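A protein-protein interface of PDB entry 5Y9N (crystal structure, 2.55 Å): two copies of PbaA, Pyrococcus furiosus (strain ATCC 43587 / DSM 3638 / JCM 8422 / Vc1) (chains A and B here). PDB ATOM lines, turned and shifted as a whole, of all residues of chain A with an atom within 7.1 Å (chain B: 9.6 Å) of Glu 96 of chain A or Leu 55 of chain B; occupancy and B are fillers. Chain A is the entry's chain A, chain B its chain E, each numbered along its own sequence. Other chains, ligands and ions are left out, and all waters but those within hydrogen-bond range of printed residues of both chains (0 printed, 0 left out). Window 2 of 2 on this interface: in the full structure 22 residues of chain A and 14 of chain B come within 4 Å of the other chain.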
ATOM      1  N   LYS A   8     -28.040  -7.764  20.512  1.00  0.00           N
ATOM      2  CA  LYS A   8     -28.312  -6.311  20.398  1.00  0.00           C
ATOM      3  C   LYS A   8     -29.715  -5.966  20.855  1.00  0.00           C
ATOM      4  O   LYS A   8     -30.655  -6.543  20.340  1.00  0.00           O
ATOM      5  CB  LYS A   8     -28.103  -5.812  18.942  1.00  0.00           C
ATOM      6  CG  LYS A   8     -26.832  -5.036  18.916  1.00  0.00           C
ATOM      7  CD  LYS A   8     -26.316  -4.484  17.588  1.00  0.00           C
ATOM      8  CE  LYS A   8     -24.893  -4.119  17.945  1.00  0.00           C
ATOM      9  NZ  LYS A   8     -24.102  -3.581  16.835  1.00  0.00           N
ATOM     10  N   PRO A   9     -29.862  -5.072  21.843  1.00  0.00           N
ATOM     11  CA  PRO A   9     -31.182  -4.869  22.461  1.00  0.00           C
ATOM     12  C   PRO A   9     -32.211  -4.140  21.622  1.00  0.00           C
ATOM     13  O   PRO A   9     -33.402  -4.337  21.827  1.00  0.00           O
ATOM     14  CB  PRO A   9     -30.846  -4.044  23.714  1.00  0.00           C
ATOM     15  CG  PRO A   9     -29.573  -3.330  23.367  1.00  0.00           C
ATOM     16  CD  PRO A   9     -28.820  -4.276  22.501  1.00  0.00           C
ATOM     17  N   VAL A  10     -31.769  -3.268  20.721  1.00  0.00           N
ATOM     18  CA  VAL A  10     -32.665  -2.441  19.914  1.00  0.00           C
ATOM     19  C   VAL A  10     -32.234  -2.478  18.451  1.00  0.00           C
ATOM     20  O   VAL A  10     -31.084  -2.174  18.119  1.00  0.00           O
ATOM     21  CB  VAL A  10     -32.642  -0.991  20.402  1.00  0.00           C
ATOM     22  CG1 VAL A  10     -33.500  -0.105  19.496  1.00  0.00           C
ATOM     23  CG2 VAL A  10     -33.114  -0.918  21.843  1.00  0.00           C
ATOM     24  N   SER A  54     -37.657  -4.241  19.733  1.00  0.00           N
ATOM     25  CA  SER A  54     -36.893  -4.601  20.914  1.00  0.00           C
ATOM     26  C   SER A  54     -37.716  -5.461  21.826  1.00  0.00           C
ATOM     27  O   SER A  54     -38.882  -5.183  22.042  1.00  0.00           O
ATOM     28  CB  SER A  54     -36.446  -3.362  21.688  1.00  0.00           C
ATOM     29  OG  SER A  54     -35.789  -3.729  22.901  1.00  0.00           O
ATOM     30  N   PHE A  56     -37.566  -5.364  24.858  1.00  0.00           N
ATOM     31  CA  PHE A  56     -37.861  -4.529  26.026  1.00  0.00           C
ATOM     32  C   PHE A  56     -38.950  -3.514  25.793  1.00  0.00           C
ATOM     33  O   PHE A  56     -39.334  -2.801  26.715  1.00  0.00           O
ATOM     34  CB  PHE A  56     -36.562  -3.871  26.516  1.00  0.00           C
ATOM     35  CG  PHE A  56     -35.480  -4.879  26.761  1.00  0.00           C
ATOM     36  CD1 PHE A  56     -35.578  -5.749  27.837  1.00  0.00           C
ATOM     37  CD2 PHE A  56     -34.432  -5.051  25.856  1.00  0.00           C
ATOM     38  CE1 PHE A  56     -34.629  -6.736  28.028  1.00  0.00           C
ATOM     39  CE2 PHE A  56     -33.498  -6.049  26.031  1.00  0.00           C
ATOM     40  CZ  PHE A  56     -33.594  -6.894  27.119  1.00  0.00           C
ATOM     41  N   PRO A  90     -38.412   3.249  29.758  1.00  0.00           N
ATOM     42  CA  PRO A  90     -37.408   3.445  30.824  1.00  0.00           C
ATOM     43  C   PRO A  90     -36.110   4.082  30.312  1.00  0.00           C
ATOM     44  O   PRO A  90     -35.757   3.895  29.148  1.00  0.00           O
ATOM     45  CB  PRO A  90     -37.171   2.028  31.377  1.00  0.00           C
ATOM     46  CG  PRO A  90     -37.780   1.076  30.380  1.00  0.00           C
ATOM     47  CD  PRO A  90     -38.686   1.835  29.457  1.00  0.00           C
ATOM     48  N   PRO A  91     -35.404   4.825  31.162  1.00  0.00           N
ATOM     49  CA  PRO A  91     -34.242   5.620  30.743  1.00  0.00           C
ATOM     50  C   PRO A  91     -33.177   4.877  29.950  1.00  0.00           C
ATOM     51  O   PRO A  91     -32.696   5.381  28.932  1.00  0.00           O
ATOM     52  CB  PRO A  91     -33.654   6.131  32.072  1.00  0.00           C
ATOM     53  CG  PRO A  91     -34.325   5.338  33.141  1.00  0.00           C
ATOM     54  CD  PRO A  91     -35.680   4.998  32.601  1.00  0.00           C
ATOM     55  N   THR A  92     -32.773   3.716  30.417  1.00  0.00           N
ATOM     56  CA  THR A  92     -31.716   2.983  29.715  1.00  0.00           C
ATOM     57  C   THR A  92     -32.134   2.588  28.293  1.00  0.00           C
ATOM     58  O   THR A  92     -31.304   2.624  27.393  1.00  0.00           O
ATOM     59  CB  THR A  92     -31.290   1.745  30.530  1.00  0.00           C
ATOM     60  OG1 THR A  92     -30.828   2.198  31.794  1.00  0.00           O
ATOM     61  CG2 THR A  92     -30.164   0.990  29.872  1.00  0.00           C
ATOM     62  N   LEU A  93     -33.406   2.235  28.102  1.00  0.00           N
ATOM     63  CA  LEU A  93     -33.906   1.854  26.790  1.00  0.00           C
ATOM     64  C   LEU A  93     -33.928   3.068  25.851  1.00  0.00           C
ATOM     65  O   LEU A  93     -33.512   2.980  24.696  1.00  0.00           O
ATOM     66  CB  LEU A  93     -35.313   1.223  26.888  1.00  0.00           C
ATOM     67  CG  LEU A  93     -35.895   0.685  25.561  1.00  0.00           C
ATOM     68  CD1 LEU A  93     -34.951  -0.345  24.911  1.00  0.00           C
ATOM     69  CD2 LEU A  93     -37.244   0.075  25.713  1.00  0.00           C
ATOM     70  N   VAL A  94     -34.398   4.195  26.369  1.00  0.00           N
ATOM     71  CA  VAL A  94     -34.332   5.468  25.656  1.00  0.00           C
ATOM     72  C   VAL A  94     -32.908   5.733  25.149  1.00  0.00           C
ATOM     73  O   VAL A  94     -32.722   6.077  23.992  1.00  0.00           O
ATOM     74  CB  VAL A  94     -34.792   6.646  26.554  1.00  0.00           C
ATOM     75  CG1 VAL A  94     -34.512   7.985  25.888  1.00  0.00           C
ATOM     76  CG2 VAL A  94     -36.275   6.541  26.879  1.00  0.00           C
ATOM     77  N   ASN A  95     -31.916   5.561  26.018  1.00  0.00           N
ATOM     78  CA  ASN A  95     -30.531   5.774  25.635  1.00  0.00           C
ATOM     79  C   ASN A  95     -30.096   4.825  24.516  1.00  0.00           C
ATOM     80  O   ASN A  95     -29.422   5.247  23.576  1.00  0.00           O
ATOM     81  CB  ASN A  95     -29.583   5.649  26.852  1.00  0.00           C
ATOM     82  CG  ASN A  95     -29.658   6.850  27.778  1.00  0.00           C
ATOM     83  OD1 ASN A  95     -30.010   7.952  27.357  1.00  0.00           O
ATOM     84  ND2 ASN A  95     -29.297   6.657  29.044  1.00  0.00           N
ATOM     85  N   GLU A  96     -30.490   3.566  24.614  1.00  0.00           N
ATOM     86  CA  GLU A  96     -30.188   2.578  23.582  1.00  0.00           C
ATOM     87  C   GLU A  96     -30.851   2.912  22.254  1.00  0.00           C
ATOM     88  O   GLU A  96     -30.237   2.771  21.203  1.00  0.00           O
ATOM     89  CB  GLU A  96     -30.540   1.163  24.065  1.00  0.00           C
ATOM     90  CG  GLU A  96     -29.518   0.699  25.085  1.00  0.00           C
ATOM     91  CD  GLU A  96     -29.838  -0.611  25.767  1.00  0.00           C
ATOM     92  OE1 GLU A  96     -28.867  -1.366  26.004  1.00  0.00           O
ATOM     93  OE2 GLU A  96     -31.017  -0.875  26.097  1.00  0.00           O
ATOM     94  N   ILE A  97     -32.084   3.389  22.299  1.00  0.00           N
ATOM     95  CA  ILE A  97     -32.755   3.803  21.083  1.00  0.00           C
ATOM     96  C   ILE A  97     -32.058   5.030  20.489  1.00  0.00           C
ATOM     97  O   ILE A  97     -31.841   5.088  19.287  1.00  0.00           O
ATOM     98  CB  ILE A  97     -34.248   4.050  21.329  1.00  0.00           C
ATOM     99  CG1 ILE A  97     -34.932   2.721  21.657  1.00  0.00           C
ATOM    100  CG2 ILE A  97     -34.909   4.694  20.109  1.00  0.00           C
ATOM    101  CD1 ILE A  97     -36.232   2.883  22.407  1.00  0.00           C
ATOM    102  N   ALA A  98     -31.691   5.983  21.335  1.00  0.00           N
ATOM    103  CA  ALA A  98     -31.004   7.190  20.883  1.00  0.00           C
ATOM    104  C   ALA A  98     -29.687   6.853  20.165  1.00  0.00           C
ATOM    105  O   ALA A  98     -29.367   7.459  19.159  1.00  0.00           O
ATOM    106  CB  ALA A  98     -30.753   8.140  22.040  1.00  0.00           C
ATOM    107  N   LYS A  99     -28.958   5.872  20.690  1.00  0.00           N
ATOM    108  CA  LYS A  99     -27.707   5.398  20.093  1.00  0.00           C
ATOM    109  C   LYS A  99     -27.978   4.936  18.656  1.00  0.00           C
ATOM    110  O   LYS A  99     -27.351   5.410  17.717  1.00  0.00           O
ATOM    111  CB  LYS A  99     -27.094   4.269  20.919  1.00  0.00           C
ATOM    112  CG  LYS A  99     -25.655   3.908  20.596  1.00  0.00           C
ATOM    113  CD  LYS A  99     -24.754   4.666  21.549  1.00  0.00           C
ATOM    114  CE  LYS A  99     -24.610   4.002  22.939  1.00  0.00           C
ATOM    115  NZ  LYS A  99     -24.311   2.526  22.975  1.00  0.00           N
ATOM    116  N   GLU A 100     -28.944   4.046  18.495  1.00  0.00           N
ATOM    117  CA  GLU A 100     -29.288   3.524  17.184  1.00  0.00           C
ATOM    118  C   GLU A 100     -29.763   4.600  16.216  1.00  0.00           C
ATOM    119  O   GLU A 100     -29.440   4.554  15.034  1.00  0.00           O
ATOM    120  CB  GLU A 100     -30.348   2.432  17.302  1.00  0.00           C
ATOM    121  CG  GLU A 100     -29.854   1.173  17.999  1.00  0.00           C
ATOM    122  CD  GLU A 100     -28.734   0.507  17.248  1.00  0.00           C
ATOM    123  OE1 GLU A 100     -28.930   0.168  16.061  1.00  0.00           O
ATOM    124  OE2 GLU A 100     -27.647   0.351  17.830  1.00  0.00           O
ATOM    125  N   ILE A 101     -30.529   5.552  16.717  1.00  0.00           N
ATOM    126  CA  ILE A 101     -31.038   6.641  15.889  1.00  0.00           C
ATOM    127  C   ILE A 101     -29.877   7.509  15.392  1.00  0.00           C
ATOM    128  O   ILE A 101     -29.829   7.828  14.224  1.00  0.00           O
ATOM    129  CB  ILE A 101     -32.078   7.506  16.639  1.00  0.00           C
ATOM    130  CG1 ILE A 101     -33.390   6.740  16.745  1.00  0.00           C
ATOM    131  CG2 ILE A 101     -32.341   8.826  15.929  1.00  0.00           C
ATOM    132  CD1 ILE A 101     -34.465   7.480  17.558  1.00  0.00           C
ATOM    133  N   MET A 159     -35.736  11.590  25.406  1.00  0.00           N
ATOM    134  CA  MET A 159     -35.168  11.403  24.085  1.00  0.00           C
ATOM    135  C   MET A 159     -34.662  12.722  23.491  1.00  0.00           C
ATOM    136  O   MET A 159     -33.609  12.783  22.878  1.00  0.00           O
ATOM    137  CB  MET A 159     -36.206  10.743  23.181  1.00  0.00           C
ATOM    138  CG  MET A 159     -35.721  10.425  21.786  1.00  0.00           C
ATOM    139  SD  MET A 159     -34.342   9.351  21.773  1.00  0.00           S
ATOM    140  CE  MET A 159     -35.143   7.793  21.729  1.00  0.00           C
ATOM    141  N   LYS A 162     -31.343  13.782  24.949  1.00  0.00           N
ATOM    142  CA  LYS A 162     -30.267  12.906  24.553  1.00  0.00           C
ATOM    143  C   LYS A 162     -29.912  13.147  23.086  1.00  0.00           C
ATOM    144  O   LYS A 162     -28.739  13.256  22.759  1.00  0.00           O
ATOM    145  CB  LYS A 162     -30.593  11.419  24.814  1.00  0.00           C
ATOM    146  CG  LYS A 162     -29.356  10.507  24.798  1.00  0.00           C
ATOM    147  CD  LYS A 162     -28.532  10.716  26.065  1.00  0.00           C
ATOM    148  CE  LYS A 162     -27.089  10.273  25.995  1.00  0.00           C
ATOM    149  NZ  LYS A 162     -27.029   8.817  26.050  1.00  0.00           N
ATOM    150  N   LYS B   8     -17.343  -1.061  27.365  1.00  0.00           N
ATOM    151  CA  LYS B   8     -17.680  -1.038  28.821  1.00  0.00           C
ATOM    152  C   LYS B   8     -18.834  -0.109  29.235  1.00  0.00           C
ATOM    153  O   LYS B   8     -19.345   0.695  28.442  1.00  0.00           O
ATOM    154  CB  LYS B   8     -16.502  -0.636  29.721  1.00  0.00           C
ATOM    155  CG  LYS B   8     -15.150  -0.741  29.140  1.00  0.00           C
ATOM    156  CD  LYS B   8     -14.613   0.616  28.719  1.00  0.00           C
ATOM    157  CE  LYS B   8     -14.177   1.503  29.850  1.00  0.00           C
ATOM    158  NZ  LYS B   8     -12.677   1.666  30.016  1.00  0.00           N
ATOM    159  N   PRO B   9     -19.296  -0.239  30.470  1.00  0.00           N
ATOM    160  CA  PRO B   9     -20.468   0.526  30.933  1.00  0.00           C
ATOM    161  C   PRO B   9     -20.278   2.030  31.133  1.00  0.00           C
ATOM    162  O   PRO B   9     -21.251   2.763  31.013  1.00  0.00           O
ATOM    163  CB  PRO B   9     -20.792  -0.129  32.276  1.00  0.00           C
ATOM    164  CG  PRO B   9     -19.539  -0.681  32.778  1.00  0.00           C
ATOM    165  CD  PRO B   9     -18.821  -1.132  31.543  1.00  0.00           C
ATOM    166  N   VAL B  10     -19.041   2.453  31.428  1.00  0.00           N
ATOM    167  CA  VAL B  10     -18.746   3.889  31.527  1.00  0.00           C
ATOM    168  C   VAL B  10     -17.516   4.259  30.701  1.00  0.00           C
ATOM    169  O   VAL B  10     -16.454   3.653  30.864  1.00  0.00           O
ATOM    170  CB  VAL B  10     -18.492   4.263  32.995  1.00  0.00           C
ATOM    171  CG1 VAL B  10     -18.114   5.735  33.109  1.00  0.00           C
ATOM    172  CG2 VAL B  10     -19.730   3.996  33.819  1.00  0.00           C
ATOM    173  N   ASN B  11     -17.686   5.263  29.846  1.00  0.00           N
ATOM    174  CA  ASN B  11     -16.599   5.823  29.046  1.00  0.00           C
ATOM    175  C   ASN B  11     -16.356   7.240  29.463  1.00  0.00           C
ATOM    176  O   ASN B  11     -17.259   8.075  29.445  1.00  0.00           O
ATOM    177  CB  ASN B  11     -16.938   5.809  27.569  1.00  0.00           C
ATOM    178  CG  ASN B  11     -17.148   4.417  27.045  1.00  0.00           C
ATOM    179  OD1 ASN B  11     -16.239   3.598  27.066  1.00  0.00           O
ATOM    180  ND2 ASN B  11     -18.350   4.138  26.580  1.00  0.00           N
ATOM    181  N   VAL B  52     -18.669  12.305  31.041  1.00  0.00           N
ATOM    182  CA  VAL B  52     -18.892  10.887  31.297  1.00  0.00           C
ATOM    183  C   VAL B  52     -20.060  10.455  30.434  1.00  0.00           C
ATOM    184  O   VAL B  52     -21.055  11.147  30.360  1.00  0.00           O
ATOM    185  CB  VAL B  52     -19.227  10.599  32.767  1.00  0.00           C
ATOM    186  CG1 VAL B  52     -19.398   9.109  32.999  1.00  0.00           C
ATOM    187  CG2 VAL B  52     -18.128  11.139  33.677  1.00  0.00           C
ATOM    188  N   ASP B  53     -19.910   9.302  29.799  1.00  0.00           N
ATOM    189  CA  ASP B  53     -20.860   8.772  28.874  1.00  0.00           C
ATOM    190  C   ASP B  53     -21.192   7.363  29.334  1.00  0.00           C
ATOM    191  O   ASP B  53     -20.288   6.557  29.540  1.00  0.00           O
ATOM    192  CB  ASP B  53     -20.242   8.718  27.496  1.00  0.00           C
ATOM    193  CG  ASP B  53     -21.228   8.212  26.445  1.00  0.00           C
ATOM    194  OD1 ASP B  53     -22.387   8.663  26.411  1.00  0.00           O
ATOM    195  OD2 ASP B  53     -20.870   7.341  25.654  1.00  0.00           O
ATOM    196  N   SER B  54     -22.480   7.079  29.498  1.00  0.00           N
ATOM    197  CA  SER B  54     -22.936   5.776  29.937  1.00  0.00           C
ATOM    198  C   SER B  54     -24.402   5.608  29.664  1.00  0.00           C
ATOM    199  O   SER B  54     -25.173   6.527  29.897  1.00  0.00           O
ATOM    200  CB  SER B  54     -22.699   5.582  31.435  1.00  0.00           C
ATOM    201  OG  SER B  54     -23.246   4.342  31.885  1.00  0.00           O
ATOM    202  N   LEU B  55     -24.783   4.418  29.231  1.00  0.00           N
ATOM    203  CA  LEU B  55     -26.188   4.071  29.038  1.00  0.00           C
ATOM    204  C   LEU B  55     -26.992   4.195  30.327  1.00  0.00           C
ATOM    205  O   LEU B  55     -28.207   4.379  30.256  1.00  0.00           O
ATOM    206  CB  LEU B  55     -26.341   2.636  28.528  1.00  0.00           C
ATOM    207  CG  LEU B  55     -25.813   2.330  27.140  1.00  0.00           C
ATOM    208  CD1 LEU B  55     -26.007   0.839  26.890  1.00  0.00           C
ATOM    209  CD2 LEU B  55     -26.497   3.191  26.066  1.00  0.00           C
ATOM    210  N   PHE B  56     -26.315   4.100  31.483  1.00  0.00           N
ATOM    211  CA  PHE B  56     -26.971   4.131  32.784  1.00  0.00           C
ATOM    212  C   PHE B  56     -27.107   5.526  33.374  1.00  0.00           C
ATOM    213  O   PHE B  56     -27.690   5.694  34.438  1.00  0.00           O
ATOM    214  CB  PHE B  56     -26.243   3.187  33.732  1.00  0.00           C
ATOM    215  CG  PHE B  56     -26.114   1.809  33.182  1.00  0.00           C
ATOM    216  CD1 PHE B  56     -27.234   1.001  33.079  1.00  0.00           C
ATOM    217  CD2 PHE B  56     -24.907   1.345  32.668  1.00  0.00           C
ATOM    218  CE1 PHE B  56     -27.140  -0.263  32.503  1.00  0.00           C
ATOM    219  CE2 PHE B  56     -24.819   0.082  32.091  1.00  0.00           C
ATOM    220  CZ  PHE B  56     -25.929  -0.713  32.016  1.00  0.00           C
ATOM    221  N   ILE B  57     -26.571   6.527  32.681  1.00  0.00           N
ATOM    222  CA  ILE B  57     -26.852   7.919  33.003  1.00  0.00           C
ATOM    223  C   ILE B  57     -28.162   8.266  32.306  1.00  0.00           C
ATOM    224  O   ILE B  57     -28.284   8.087  31.095  1.00  0.00           O
ATOM    225  CB  ILE B  57     -25.731   8.882  32.539  1.00  0.00           C
ATOM    226  CG1 ILE B  57     -24.495   8.666  33.417  1.00  0.00           C
ATOM    227  CG2 ILE B  57     -26.173  10.340  32.651  1.00  0.00           C
ATOM    228  CD1 ILE B  57     -23.235   9.306  32.895  1.00  0.00           C
ATOM    229  N   PRO B  58     -29.143   8.767  33.067  1.00  0.00           N
ATOM    230  CA  PRO B  58     -30.425   8.984  32.443  1.00  0.00           C
ATOM    231  C   PRO B  58     -30.357  10.054  31.370  1.00  0.00           C
ATOM    232  O   PRO B  58     -29.619  11.003  31.520  1.00  0.00           O
ATOM    233  CB  PRO B  58     -31.357   9.382  33.607  1.00  0.00           C
ATOM    234  CG  PRO B  58     -30.505   9.636  34.764  1.00  0.00           C
ATOM    235  CD  PRO B  58     -29.183   8.979  34.524  1.00  0.00           C
ATOM    236  N   PRO B  59     -31.152   9.896  30.313  1.00  0.00           N
ATOM    237  CA  PRO B  59     -31.120  10.798  29.167  1.00  0.00           C
ATOM    238  C   PRO B  59     -31.517  12.201  29.545  1.00  0.00           C
ATOM    239  O   PRO B  59     -32.607  12.410  30.058  1.00  0.00           O
ATOM    240  CB  PRO B  59     -32.178  10.212  28.225  1.00  0.00           C
ATOM    241  CG  PRO B  59     -33.130   9.473  29.116  1.00  0.00           C
ATOM    242  CD  PRO B  59     -32.302   8.955  30.260  1.00  0.00           C
ATOM    243  N   MET B  60     -30.620  13.149  29.307  1.00  0.00           N
ATOM    244  CA  MET B  60     -30.926  14.575  29.425  1.00  0.00           C
ATOM    245  C   MET B  60     -29.820  15.406  28.812  1.00  0.00           C
ATOM    246  O   MET B  60     -28.707  14.920  28.622  1.00  0.00           O
ATOM    247  CB  MET B  60     -31.087  14.997  30.886  1.00  0.00           C
ATOM    248  CG  MET B  60     -29.819  14.918  31.709  1.00  0.00           C
ATOM    249  SD  MET B  60     -30.164  14.687  33.473  1.00  0.00           S
ATOM    250  CE  MET B  60     -30.618  16.350  33.923  1.00  0.00           C
ATOM    251  N   LEU B  89     -26.427   9.629  41.613  1.00  0.00           N
ATOM    252  CA  LEU B  89     -26.273   8.423  40.834  1.00  0.00           C
ATOM    253  C   LEU B  89     -26.279   7.222  41.743  1.00  0.00           C
ATOM    254  O   LEU B  89     -25.855   7.309  42.891  1.00  0.00           O
ATOM    255  CB  LEU B  89     -24.942   8.469  40.121  1.00  0.00           C
ATOM    256  CG  LEU B  89     -24.858   9.491  38.993  1.00  0.00           C
ATOM    257  CD1 LEU B  89     -23.448  10.066  38.943  1.00  0.00           C
ATOM    258  CD2 LEU B  89     -25.290   8.866  37.668  1.00  0.00           C
ATOM    259  N   PRO B  90     -26.729   6.076  41.218  1.00  0.00           N
ATOM    260  CA  PRO B  90     -26.724   4.875  42.065  1.00  0.00           C
ATOM    261  C   PRO B  90     -25.317   4.393  42.418  1.00  0.00           C
ATOM    262  O   PRO B  90     -24.390   4.603  41.641  1.00  0.00           O
ATOM    263  CB  PRO B  90     -27.501   3.835  41.240  1.00  0.00           C
ATOM    264  CG  PRO B  90     -27.620   4.396  39.865  1.00  0.00           C
ATOM    265  CD  PRO B  90     -27.270   5.843  39.873  1.00  0.00           C
ATOM    266  N   LEU B  93     -22.850   2.575  39.931  1.00  0.00           N
ATOM    267  CA  LEU B  93     -22.442   3.431  38.818  1.00  0.00           C
ATOM    268  C   LEU B  93     -21.352   4.412  39.272  1.00  0.00           C
ATOM    269  O   LEU B  93     -20.355   4.607  38.582  1.00  0.00           O
ATOM    270  CB  LEU B  93     -23.640   4.179  38.219  1.00  0.00           C
ATOM    271  CG  LEU B  93     -23.347   5.032  36.974  1.00  0.00           C
ATOM    272  CD1 LEU B  93     -22.720   4.201  35.861  1.00  0.00           C
ATOM    273  CD2 LEU B  93     -24.600   5.726  36.459  1.00  0.00           C
ATOM    274  N   GLU B  96     -18.156   2.576  39.297  1.00  0.00           N
ATOM    275  CA  GLU B  96     -17.664   2.419  37.938  1.00  0.00           C
ATOM    276  C   GLU B  96     -17.065   3.703  37.383  1.00  0.00           C
ATOM    277  O   GLU B  96     -16.020   3.674  36.730  1.00  0.00           O
ATOM    278  CB  GLU B  96     -18.761   1.852  37.028  1.00  0.00           C
ATOM    279  CG  GLU B  96     -18.984   0.382  37.326  1.00  0.00           C
ATOM    280  CD  GLU B  96     -20.162  -0.227  36.577  1.00  0.00           C
ATOM    281  OE1 GLU B  96     -20.021  -1.363  36.042  1.00  0.00           O
ATOM    282  OE2 GLU B  96     -21.235   0.380  36.484  1.00  0.00           O
ATOM    283  N   ILE B  97     -17.690   4.831  37.678  1.00  0.00           N
ATOM    284  CA  ILE B  97     -17.147   6.106  37.253  1.00  0.00           C
ATOM    285  C   ILE B  97     -15.826   6.379  37.983  1.00  0.00           C
ATOM    286  O   ILE B  97     -14.864   6.818  37.358  1.00  0.00           O
ATOM    287  CB  ILE B  97     -18.157   7.240  37.465  1.00  0.00           C
ATOM    288  CG1 ILE B  97     -19.336   7.037  36.498  1.00  0.00           C
ATOM    289  CG2 ILE B  97     -17.519   8.604  37.231  1.00  0.00           C
ATOM    290  CD1 ILE B  97     -20.600   7.748  36.938  1.00  0.00           C
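The side-chain amide nitrogen (ND2) of Asn 95 of chain A is in hydrogen-bond range of the backbone carbonyl oxygen (O) of Leu 55 of chain B (2.8 Å). O of Ile 57 of chain B sits at hydrogen-bond distance from ND2 of Asn 95 of chain A (2.7 Å).
Among the printed residues, pairs that only touch across the chains: Pro 91 of chain A with Pro 59 of chain B (3.6 Å), Thr 92 of chain A with Leu 55 of chain B (3.7 Å), Val 94 of chain A with Pro 59 of chain B (3.8 Å), Asn 95 of chain A with Pro 59 of chain B (3.2 Å), Glu 96 of chain A with Leu 55 of chain B (3.7 Å), Lys 99 of chain A with Leu 55 of chain B (3.7 Å) and Lys 162 of chain A with Pro 59 of chain B (3.95 Å).
Of the 18 printed residues of chain B, 3 touch a printed residue of chain A. Hydrophobic or aromatic side chains of chain B that line the printed part of chain A: Leu 55 and Pro 59. Of the 19 printed residues of chain A, 7 touch a printed residue of chain B. Printed residues of chain A that touch a printed residue of chain B: Pro 91, Thr 92, Val 94, Asn 95, Glu 96, Lys 99 and Lys 162. Hydrophobic or aromatic side chains of chain A that line the printed part of chain B: Pro 91 and Val 94. Among the printed residues, no Asp or Glu carboxylate lies within 4 Å of a Lys or Arg side-chain nitrogen of the other chain.
Of the printed residues of chain B, Pro 91 of chain A touches Pro 59 (3.6 Å). Of the printed residues of chain B, Val 94 of chain A touches Pro 59. Of the printed residues of chain B, Asn 95 of chain A touches Leu 55, Ile 57 and Pro 59. Glu 96 of chain A touches just one residue of chain B: Leu 55. Ile 97 of chain A touches none of the printed residues of chain B. Of chain B, only Leu 55 (3.7 Å) comes within 4 Å of Lys 99 of chain A. Printed residues of chain B within 4 Å of Lys 162 of chain A: Pro 59. Leu 55 of chain B touches four residues of chain A. Of the printed residues of chain A, Ile 57 of chain B touches Asn 95. Of the printed residues of chain A, Pro 59 of chain B touches Pro 91, Val 94, Asn 95 and Lys 162. The nearest residue of chain B that does not touch Glu 96 of chain A is Phe 56 of chain B (6.7 Å).
Positions printed for both chains: 8, 9, 10, 54, 56, 90, 93, 96 and 97. Of the 9 pairs that touch across the chains among the printed residues, none has its exchanged pair printed and touching as well.
The side-chain amino group of Lys 162 of chain A lies within hydrogen-bond range of the side-chain amide oxygen of Asn 95 of chain A, at 3.4 Å.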
